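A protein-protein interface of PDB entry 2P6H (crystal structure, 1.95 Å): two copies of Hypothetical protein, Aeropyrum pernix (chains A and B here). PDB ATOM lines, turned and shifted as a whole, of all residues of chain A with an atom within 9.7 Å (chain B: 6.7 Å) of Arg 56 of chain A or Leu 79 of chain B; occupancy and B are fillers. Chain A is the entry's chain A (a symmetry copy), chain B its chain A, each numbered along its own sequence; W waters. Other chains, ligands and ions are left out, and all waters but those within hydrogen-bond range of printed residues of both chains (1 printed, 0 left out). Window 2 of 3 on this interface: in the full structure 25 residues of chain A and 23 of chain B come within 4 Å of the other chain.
NZ of Lys 76 of chain B lies within salt-bridge range of OE1 of Glu 59 of chain A, at 2.9 Å. The backbone NH (N) of Lys 76 of chain B sits at hydrogen-bond distance from the side-chain carboxylate (OD1) of Asp 60 of chain A (2.8 Å). A ring nitrogen (ND1) of His 77 of chain B lies within hydrogen-bond range of the side-chain carboxylate (OE1) of Glu 54 of chain A, at 2.8 Å. The backbone NH (N) of His 77 of chain B lies within hydrogen-bond range of the side-chain carboxylate (OD2) of Asp 60 of chain A (2.8 Å).
The backbone carbonyl oxygen (O) of Trp 75 of chain B sits close to the side-chain amide oxygen (OD1) of Asn 78 of chain B (3.3 Å). The side-chain carboxylate (OE2) of Glu 54 of chain A is in salt-bridge range of the guanidinium group (NH1) of Arg 56 of chain A (3.0 Å). OE1 of Glu 54 of chain A sits at hydrogen-bond distance from N of Leu 57 of chain A (2.8 Å).
CG2 of Val 80 of chain B touches OE2 of Glu 54 of chain A, at 3.9 Å. Lys 76 of chain B touches Arg 56 of chain A. His 77 of chain B touches Arg 56 of chain A (N to CB, 3.9 Å). Arg 56 of chain A touches Leu 79 of chain B. Val 80 of chain B touches Arg 56 of chain A. Leu 57 of chain A touches His 77 of chain B (CB to ND1, 3.8 Å). Trp 75 of chain B touches Asp 60 of chain A.
Of the printed residues of chain B, Glu 54 of chain A touches His 77 and Val 80. Arg 56 of chain A touches just these residues of chain B: Lys 76 (3.7 Å), His 77 (3.9 Å), Leu 79 (3.7 Å) and Val 80 (3.2 Å). Of the printed residues of chain B, Glu 59 of chain A touches Lys 76 (2.9 Å). Ile 61 of chain A touches none of the printed residues of chain B. Of the printed residues of chain A, Trp 75 of chain B touches Asp 60. Of the printed residues of chain A, Lys 76 of chain B touches Arg 56, Glu 59 and Asp 60. The nearest residue of chain A that does not touch Leu 79 of chain B is Glu 54 of chain A (6.8 Å).
Printed residues of chain B that touch a printed residue of chain A: Trp 75, Lys 76, His 77, Leu 79 and Val 80. Hydrophobic or aromatic side chains of chain B that line the printed part of chain A: Trp 75, His 77, Leu 79 and Val 80. Among the printed residues, 11 pairs touch across the chains. Among the printed residues, Asp or Glu carboxylates within 4 Å of a Lys or Arg side-chain nitrogen of the other chain: Glu 59 of chain A with Lys 76 of chain B.
No position is printed for both chains. Of the 11 pairs that touch across the chains among the printed residues, none has its exchanged pair printed and touching as well.
Water W1 bridges OE1 of Glu 52 of chain A (2.9 Å) and NE2 of His 77 of chain B (3.3 Å).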
ATOM      1  N   VAL A  16      -7.043 -21.518 -13.055  1.00  0.00           N
ATOM      2  CA  VAL A  16      -5.961 -22.095 -12.272  1.00  0.00           C
ATOM      3  C   VAL A  16      -4.954 -20.984 -12.024  1.00  0.00           C
ATOM      4  O   VAL A  16      -4.555 -20.296 -12.970  1.00  0.00           O
ATOM      5  CB  VAL A  16      -5.275 -23.245 -13.027  1.00  0.00           C
ATOM      6  CG1 VAL A  16      -4.068 -23.732 -12.241  1.00  0.00           C
ATOM      7  CG2 VAL A  16      -6.256 -24.380 -13.269  1.00  0.00           C
ATOM      8  N   GLU A  52       2.798 -28.267 -12.768  1.00  0.00           N
ATOM      9  CA  GLU A  52       3.561 -27.260 -13.504  1.00  0.00           C
ATOM     10  C   GLU A  52       2.737 -26.034 -13.880  1.00  0.00           C
ATOM     11  O   GLU A  52       1.622 -26.155 -14.404  1.00  0.00           O
ATOM     12  CB  GLU A  52       4.162 -27.887 -14.770  1.00  0.00           C
ATOM     13  CG  GLU A  52       5.317 -27.097 -15.356  1.00  0.00           C
ATOM     14  CD  GLU A  52       5.995 -27.793 -16.542  1.00  0.00           C
ATOM     15  OE1 GLU A  52       5.934 -29.051 -16.645  1.00  0.00           O
ATOM     16  OE2 GLU A  52       6.608 -27.076 -17.365  1.00  0.00           O
ATOM     17  N   ALA A  53       3.291 -24.852 -13.620  1.00  0.00           N
ATOM     18  CA  ALA A  53       2.589 -23.606 -13.931  1.00  0.00           C
ATOM     19  C   ALA A  53       2.885 -23.135 -15.370  1.00  0.00           C
ATOM     20  O   ALA A  53       3.253 -21.994 -15.615  1.00  0.00           O
ATOM     21  CB  ALA A  53       2.982 -22.532 -12.887  1.00  0.00           C
ATOM     22  N   GLU A  54       2.720 -24.023 -16.343  1.00  0.00           N
ATOM     23  CA  GLU A  54       2.898 -23.659 -17.716  1.00  0.00           C
ATOM     24  C   GLU A  54       1.577 -23.155 -18.220  1.00  0.00           C
ATOM     25  O   GLU A  54       0.541 -23.790 -18.067  1.00  0.00           O
ATOM     26  CB  GLU A  54       3.311 -24.904 -18.498  1.00  0.00           C
ATOM     27  CG  GLU A  54       3.880 -24.562 -19.877  1.00  0.00           C
ATOM     28  CD  GLU A  54       2.752 -24.440 -20.879  1.00  0.00           C
ATOM     29  OE1 GLU A  54       1.985 -25.382 -21.016  1.00  0.00           O
ATOM     30  OE2 GLU A  54       2.670 -23.407 -21.544  1.00  0.00           O
ATOM     31  N   PRO A  55       1.526 -21.933 -18.799  1.00  0.00           N
ATOM     32  CA  PRO A  55       0.253 -21.359 -19.285  1.00  0.00           C
ATOM     33  C   PRO A  55      -0.704 -22.251 -20.074  1.00  0.00           C
ATOM     34  O   PRO A  55      -1.884 -22.339 -19.747  1.00  0.00           O
ATOM     35  CB  PRO A  55       0.686 -20.095 -20.069  1.00  0.00           C
ATOM     36  CG  PRO A  55       2.200 -20.266 -20.229  1.00  0.00           C
ATOM     37  CD  PRO A  55       2.622 -20.959 -18.951  1.00  0.00           C
ATOM     38  N   ARG A  56      -0.199 -22.938 -21.086  1.00  0.00           N
ATOM     39  CA  ARG A  56      -1.087 -23.771 -21.875  1.00  0.00           C
ATOM     40  C   ARG A  56      -1.614 -24.936 -21.044  1.00  0.00           C
ATOM     41  O   ARG A  56      -2.796 -25.252 -21.049  1.00  0.00           O
ATOM     42  CB  ARG A  56      -0.302 -24.299 -23.076  1.00  0.00           C
ATOM     43  CG  ARG A  56      -0.077 -23.222 -24.137  1.00  0.00           C
ATOM     44  CD  ARG A  56       1.163 -23.507 -24.993  1.00  0.00           C
ATOM     45  NE  ARG A  56       1.589 -22.293 -25.696  1.00  0.00           N
ATOM     46  CZ  ARG A  56       2.710 -21.689 -25.257  1.00  0.00           C
ATOM     47  NH1 ARG A  56       3.384 -22.198 -24.242  1.00  0.00           N
ATOM     48  NH2 ARG A  56       3.127 -20.566 -25.846  1.00  0.00           N
ATOM     49  N   LEU A  57      -0.747 -25.570 -20.258  1.00  0.00           N
ATOM     50  CA  LEU A  57      -1.173 -26.663 -19.371  1.00  0.00           C
ATOM     51  C   LEU A  57      -2.284 -26.204 -18.433  1.00  0.00           C
ATOM     52  O   LEU A  57      -3.223 -26.932 -18.137  1.00  0.00           O
ATOM     53  CB  LEU A  57       0.028 -27.166 -18.546  1.00  0.00           C
ATOM     54  CG  LEU A  57      -0.344 -28.252 -17.505  1.00  0.00           C
ATOM     55  CD1 LEU A  57      -0.936 -29.502 -18.155  1.00  0.00           C
ATOM     56  CD2 LEU A  57       0.857 -28.722 -16.684  1.00  0.00           C
ATOM     57  N   MET A  58      -2.158 -24.981 -17.942  1.00  0.00           N
ATOM     58  CA  MET A  58      -3.136 -24.452 -17.004  1.00  0.00           C
ATOM     59  C   MET A  58      -4.493 -24.298 -17.676  1.00  0.00           C
ATOM     60  O   MET A  58      -5.535 -24.427 -17.030  1.00  0.00           O
ATOM     61  CB  MET A  58      -2.627 -23.131 -16.436  1.00  0.00           C
ATOM     62  CG  MET A  58      -1.428 -23.347 -15.516  1.00  0.00           C
ATOM     63  SD  MET A  58      -0.522 -21.850 -15.134  1.00  0.00           S
ATOM     64  CE  MET A  58      -1.743 -20.955 -14.153  1.00  0.00           C
ATOM     65  N   GLU A  59      -4.475 -24.024 -18.977  1.00  0.00           N
ATOM     66  CA  GLU A  59      -5.701 -23.946 -19.766  1.00  0.00           C
ATOM     67  C   GLU A  59      -6.255 -25.331 -19.888  1.00  0.00           C
ATOM     68  O   GLU A  59      -7.452 -25.559 -19.779  1.00  0.00           O
ATOM     69  CB  GLU A  59      -5.444 -23.401 -21.190  1.00  0.00           C
ATOM     70  CG  GLU A  59      -5.506 -21.874 -21.241  1.00  0.00           C
ATOM     71  CD  GLU A  59      -5.416 -21.415 -22.678  1.00  0.00           C
ATOM     72  OE1 GLU A  59      -6.457 -21.329 -23.327  1.00  0.00           O
ATOM     73  OE2 GLU A  59      -4.317 -21.144 -23.141  1.00  0.00           O
ATOM     74  N   ASP A  60      -5.364 -26.286 -20.141  1.00  0.00           N
ATOM     75  CA  ASP A  60      -5.790 -27.672 -20.317  1.00  0.00           C
ATOM     76  C   ASP A  60      -6.460 -28.225 -19.054  1.00  0.00           C
ATOM     77  O   ASP A  60      -7.384 -29.005 -19.095  1.00  0.00           O
ATOM     78  CB  ASP A  60      -4.581 -28.557 -20.641  1.00  0.00           C
ATOM     79  CG  ASP A  60      -4.051 -28.310 -22.060  1.00  0.00           C
ATOM     80  OD1 ASP A  60      -4.817 -27.842 -22.902  1.00  0.00           O
ATOM     81  OD2 ASP A  60      -2.894 -28.635 -22.290  1.00  0.00           O
ATOM     82  N   ILE A  61      -5.892 -27.810 -17.891  1.00  0.00           N
ATOM     83  CA  ILE A  61      -6.471 -28.286 -16.652  1.00  0.00           C
ATOM     84  C   ILE A  61      -7.921 -27.840 -16.503  1.00  0.00           C
ATOM     85  O   ILE A  61      -8.798 -28.588 -16.091  1.00  0.00           O
ATOM     86  CB  ILE A  61      -5.609 -27.735 -15.537  1.00  0.00           C
ATOM     87  CG1 ILE A  61      -4.268 -28.497 -15.551  1.00  0.00           C
ATOM     88  CG2 ILE A  61      -6.339 -27.970 -14.192  1.00  0.00           C
ATOM     89  CD1 ILE A  61      -3.248 -28.140 -14.464  1.00  0.00           C
ATOM     90  N   VAL A  62      -8.180 -26.574 -16.861  1.00  0.00           N
ATOM     91  CA  VAL A  62      -9.549 -26.123 -16.794  1.00  0.00           C
ATOM     92  C   VAL A  62     -10.447 -26.883 -17.756  1.00  0.00           C
ATOM     93  O   VAL A  62     -11.556 -27.284 -17.427  1.00  0.00           O
ATOM     94  CB  VAL A  62      -9.519 -24.688 -17.221  1.00  0.00           C
ATOM     95  CG1 VAL A  62     -10.915 -24.246 -17.655  1.00  0.00           C
ATOM     96  CG2 VAL A  62      -9.056 -23.815 -16.071  1.00  0.00           C
ATOM     97  N   GLU A  63      -9.971 -27.093 -18.992  1.00  0.00           N
ATOM     98  CA  GLU A  63     -10.780 -27.837 -19.945  1.00  0.00           C
ATOM     99  C   GLU A  63     -11.002 -29.289 -19.500  1.00  0.00           C
ATOM    100  O   GLU A  63     -12.071 -29.856 -19.692  1.00  0.00           O
ATOM    101  CB  GLU A  63     -10.107 -27.799 -21.314  1.00  0.00           C
ATOM    102  CG  GLU A  63     -10.857 -28.623 -22.366  1.00  0.00           C
ATOM    103  CD  GLU A  63     -12.235 -28.044 -22.651  1.00  0.00           C
ATOM    104  OE1 GLU A  63     -12.473 -26.865 -22.339  1.00  0.00           O
ATOM    105  OE2 GLU A  63     -13.056 -28.769 -23.207  1.00  0.00           O
ATOM    106  N   PHE A  64      -9.977 -29.887 -18.903  1.00  0.00           N
ATOM    107  CA  PHE A  64     -10.063 -31.259 -18.405  1.00  0.00           C
ATOM    108  C   PHE A  64     -11.166 -31.339 -17.356  1.00  0.00           C
ATOM    109  O   PHE A  64     -12.006 -32.218 -17.352  1.00  0.00           O
ATOM    110  CB  PHE A  64      -8.693 -31.639 -17.808  1.00  0.00           C
ATOM    111  CG  PHE A  64      -8.680 -32.989 -17.108  1.00  0.00           C
ATOM    112  CD1 PHE A  64      -8.938 -34.155 -17.818  1.00  0.00           C
ATOM    113  CD2 PHE A  64      -8.323 -33.056 -15.768  1.00  0.00           C
ATOM    114  CE1 PHE A  64      -8.842 -35.390 -17.176  1.00  0.00           C
ATOM    115  CE2 PHE A  64      -8.228 -34.295 -15.132  1.00  0.00           C
ATOM    116  CZ  PHE A  64      -8.485 -35.464 -15.834  1.00  0.00           C
ATOM    117  N   TRP B  75      -4.793 -31.323 -26.454  1.00  0.00           N
ATOM    118  CA  TRP B  75      -4.377 -30.492 -25.330  1.00  0.00           C
ATOM    119  C   TRP B  75      -3.463 -29.394 -25.859  1.00  0.00           C
ATOM    120  O   TRP B  75      -2.601 -29.651 -26.698  1.00  0.00           O
ATOM    121  CB  TRP B  75      -3.618 -31.331 -24.297  1.00  0.00           C
ATOM    122  CG  TRP B  75      -4.426 -32.459 -23.744  1.00  0.00           C
ATOM    123  CD1 TRP B  75      -4.155 -33.799 -23.843  1.00  0.00           C
ATOM    124  CD2 TRP B  75      -5.646 -32.349 -23.013  1.00  0.00           C
ATOM    125  NE1 TRP B  75      -5.139 -34.527 -23.214  1.00  0.00           N
ATOM    126  CE2 TRP B  75      -6.065 -33.660 -22.694  1.00  0.00           C
ATOM    127  CE3 TRP B  75      -6.430 -31.266 -22.593  1.00  0.00           C
ATOM    128  CZ2 TRP B  75      -7.236 -33.916 -21.977  1.00  0.00           C
ATOM    129  CZ3 TRP B  75      -7.595 -31.520 -21.880  1.00  0.00           C
ATOM    130  CH2 TRP B  75      -7.984 -32.840 -21.577  1.00  0.00           C
ATOM    131  N   LYS B  76      -3.653 -28.174 -25.372  1.00  0.00           N
ATOM    132  CA  LYS B  76      -2.833 -27.057 -25.831  1.00  0.00           C
ATOM    133  C   LYS B  76      -1.375 -27.189 -25.380  1.00  0.00           C
ATOM    134  O   LYS B  76      -0.459 -26.644 -25.981  1.00  0.00           O
ATOM    135  CB  LYS B  76      -3.429 -25.768 -25.270  1.00  0.00           C
ATOM    136  CG  LYS B  76      -4.740 -25.394 -25.960  1.00  0.00           C
ATOM    137  CD  LYS B  76      -5.433 -24.217 -25.276  1.00  0.00           C
ATOM    138  CE  LYS B  76      -6.247 -23.373 -26.261  1.00  0.00           C
ATOM    139  NZ  LYS B  76      -7.432 -22.841 -25.592  1.00  0.00           N
ATOM    140  N   HIS B  77      -1.141 -27.932 -24.301  1.00  0.00           N
ATOM    141  CA  HIS B  77       0.219 -28.164 -23.819  1.00  0.00           C
ATOM    142  C   HIS B  77       0.993 -28.916 -24.917  1.00  0.00           C
ATOM    143  O   HIS B  77       2.222 -28.930 -24.902  1.00  0.00           O
ATOM    144  CB  HIS B  77       0.206 -28.997 -22.531  1.00  0.00           C
ATOM    145  CG  HIS B  77       1.553 -29.185 -21.908  1.00  0.00           C
ATOM    146  ND1 HIS B  77       2.332 -28.133 -21.458  1.00  0.00           N
ATOM    147  CD2 HIS B  77       2.260 -30.308 -21.629  1.00  0.00           C
ATOM    148  CE1 HIS B  77       3.444 -28.601 -20.933  1.00  0.00           C
ATOM    149  NE2 HIS B  77       3.427 -29.924 -21.025  1.00  0.00           N
ATOM    150  N   ASN B  78       0.271 -29.526 -25.867  1.00  0.00           N
ATOM    151  CA  ASN B  78       0.914 -30.280 -27.008  1.00  0.00           C
ATOM    152  C   ASN B  78       1.824 -29.400 -27.810  1.00  0.00           C
ATOM    153  O   ASN B  78       2.734 -29.860 -28.486  1.00  0.00           O
ATOM    154  CB  ASN B  78      -0.069 -30.865 -28.050  1.00  0.00           C
ATOM    155  CG  ASN B  78      -0.835 -32.002 -27.424  1.00  0.00           C
ATOM    156  OD1 ASN B  78      -0.714 -32.290 -26.235  1.00  0.00           O
ATOM    157  ND2 ASN B  78      -1.642 -32.674 -28.261  1.00  0.00           N
ATOM    158  N   LEU B  79       1.590 -28.097 -27.809  1.00  0.00           N
ATOM    159  CA  LEU B  79       2.468 -27.201 -28.567  1.00  0.00           C
ATOM    160  C   LEU B  79       3.842 -27.198 -27.905  1.00  0.00           C
ATOM    161  O   LEU B  79       4.865 -27.044 -28.568  1.00  0.00           O
ATOM    162  CB  LEU B  79       1.832 -25.800 -28.560  1.00  0.00           C
ATOM    163  CG  LEU B  79       2.645 -24.687 -29.225  1.00  0.00           C
ATOM    164  CD1 LEU B  79       1.708 -23.578 -29.738  1.00  0.00           C
ATOM    165  CD2 LEU B  79       3.634 -24.042 -28.240  1.00  0.00           C
ATOM    166  N   VAL B  80       3.827 -27.393 -26.569  1.00  0.00           N
ATOM    167  CA  VAL B  80       5.051 -27.334 -25.746  1.00  0.00           C
ATOM    168  C   VAL B  80       5.735 -28.714 -25.551  1.00  0.00           C
ATOM    169  O   VAL B  80       6.950 -28.855 -25.632  1.00  0.00           O
ATOM    170  CB  VAL B  80       4.698 -26.678 -24.392  1.00  0.00           C
ATOM    171  CG1 VAL B  80       5.877 -26.775 -23.420  1.00  0.00           C
ATOM    172  CG2 VAL B  80       4.351 -25.207 -24.590  1.00  0.00           C
ATOM    173  N   ASP B  81       4.941 -29.745 -25.246  1.00  0.00           N
ATOM    174  CA  ASP B  81       5.520 -31.062 -24.984  1.00  0.00           C
ATOM    175  C   ASP B  81       4.477 -32.115 -25.341  1.00  0.00           C
ATOM    176  O   ASP B  81       3.427 -31.783 -25.877  1.00  0.00           O
ATOM    177  CB  ASP B  81       5.881 -31.136 -23.484  1.00  0.00           C
ATOM    178  CG  ASP B  81       7.013 -32.120 -23.201  1.00  0.00           C
ATOM    179  OD1 ASP B  81       7.266 -33.011 -24.028  1.00  0.00           O
ATOM    180  OD2 ASP B  81       7.626 -32.008 -22.129  1.00  0.00           O
HETATM  181  O   HOH W   1       6.037 -30.507 -19.134  1.00  0.00           O
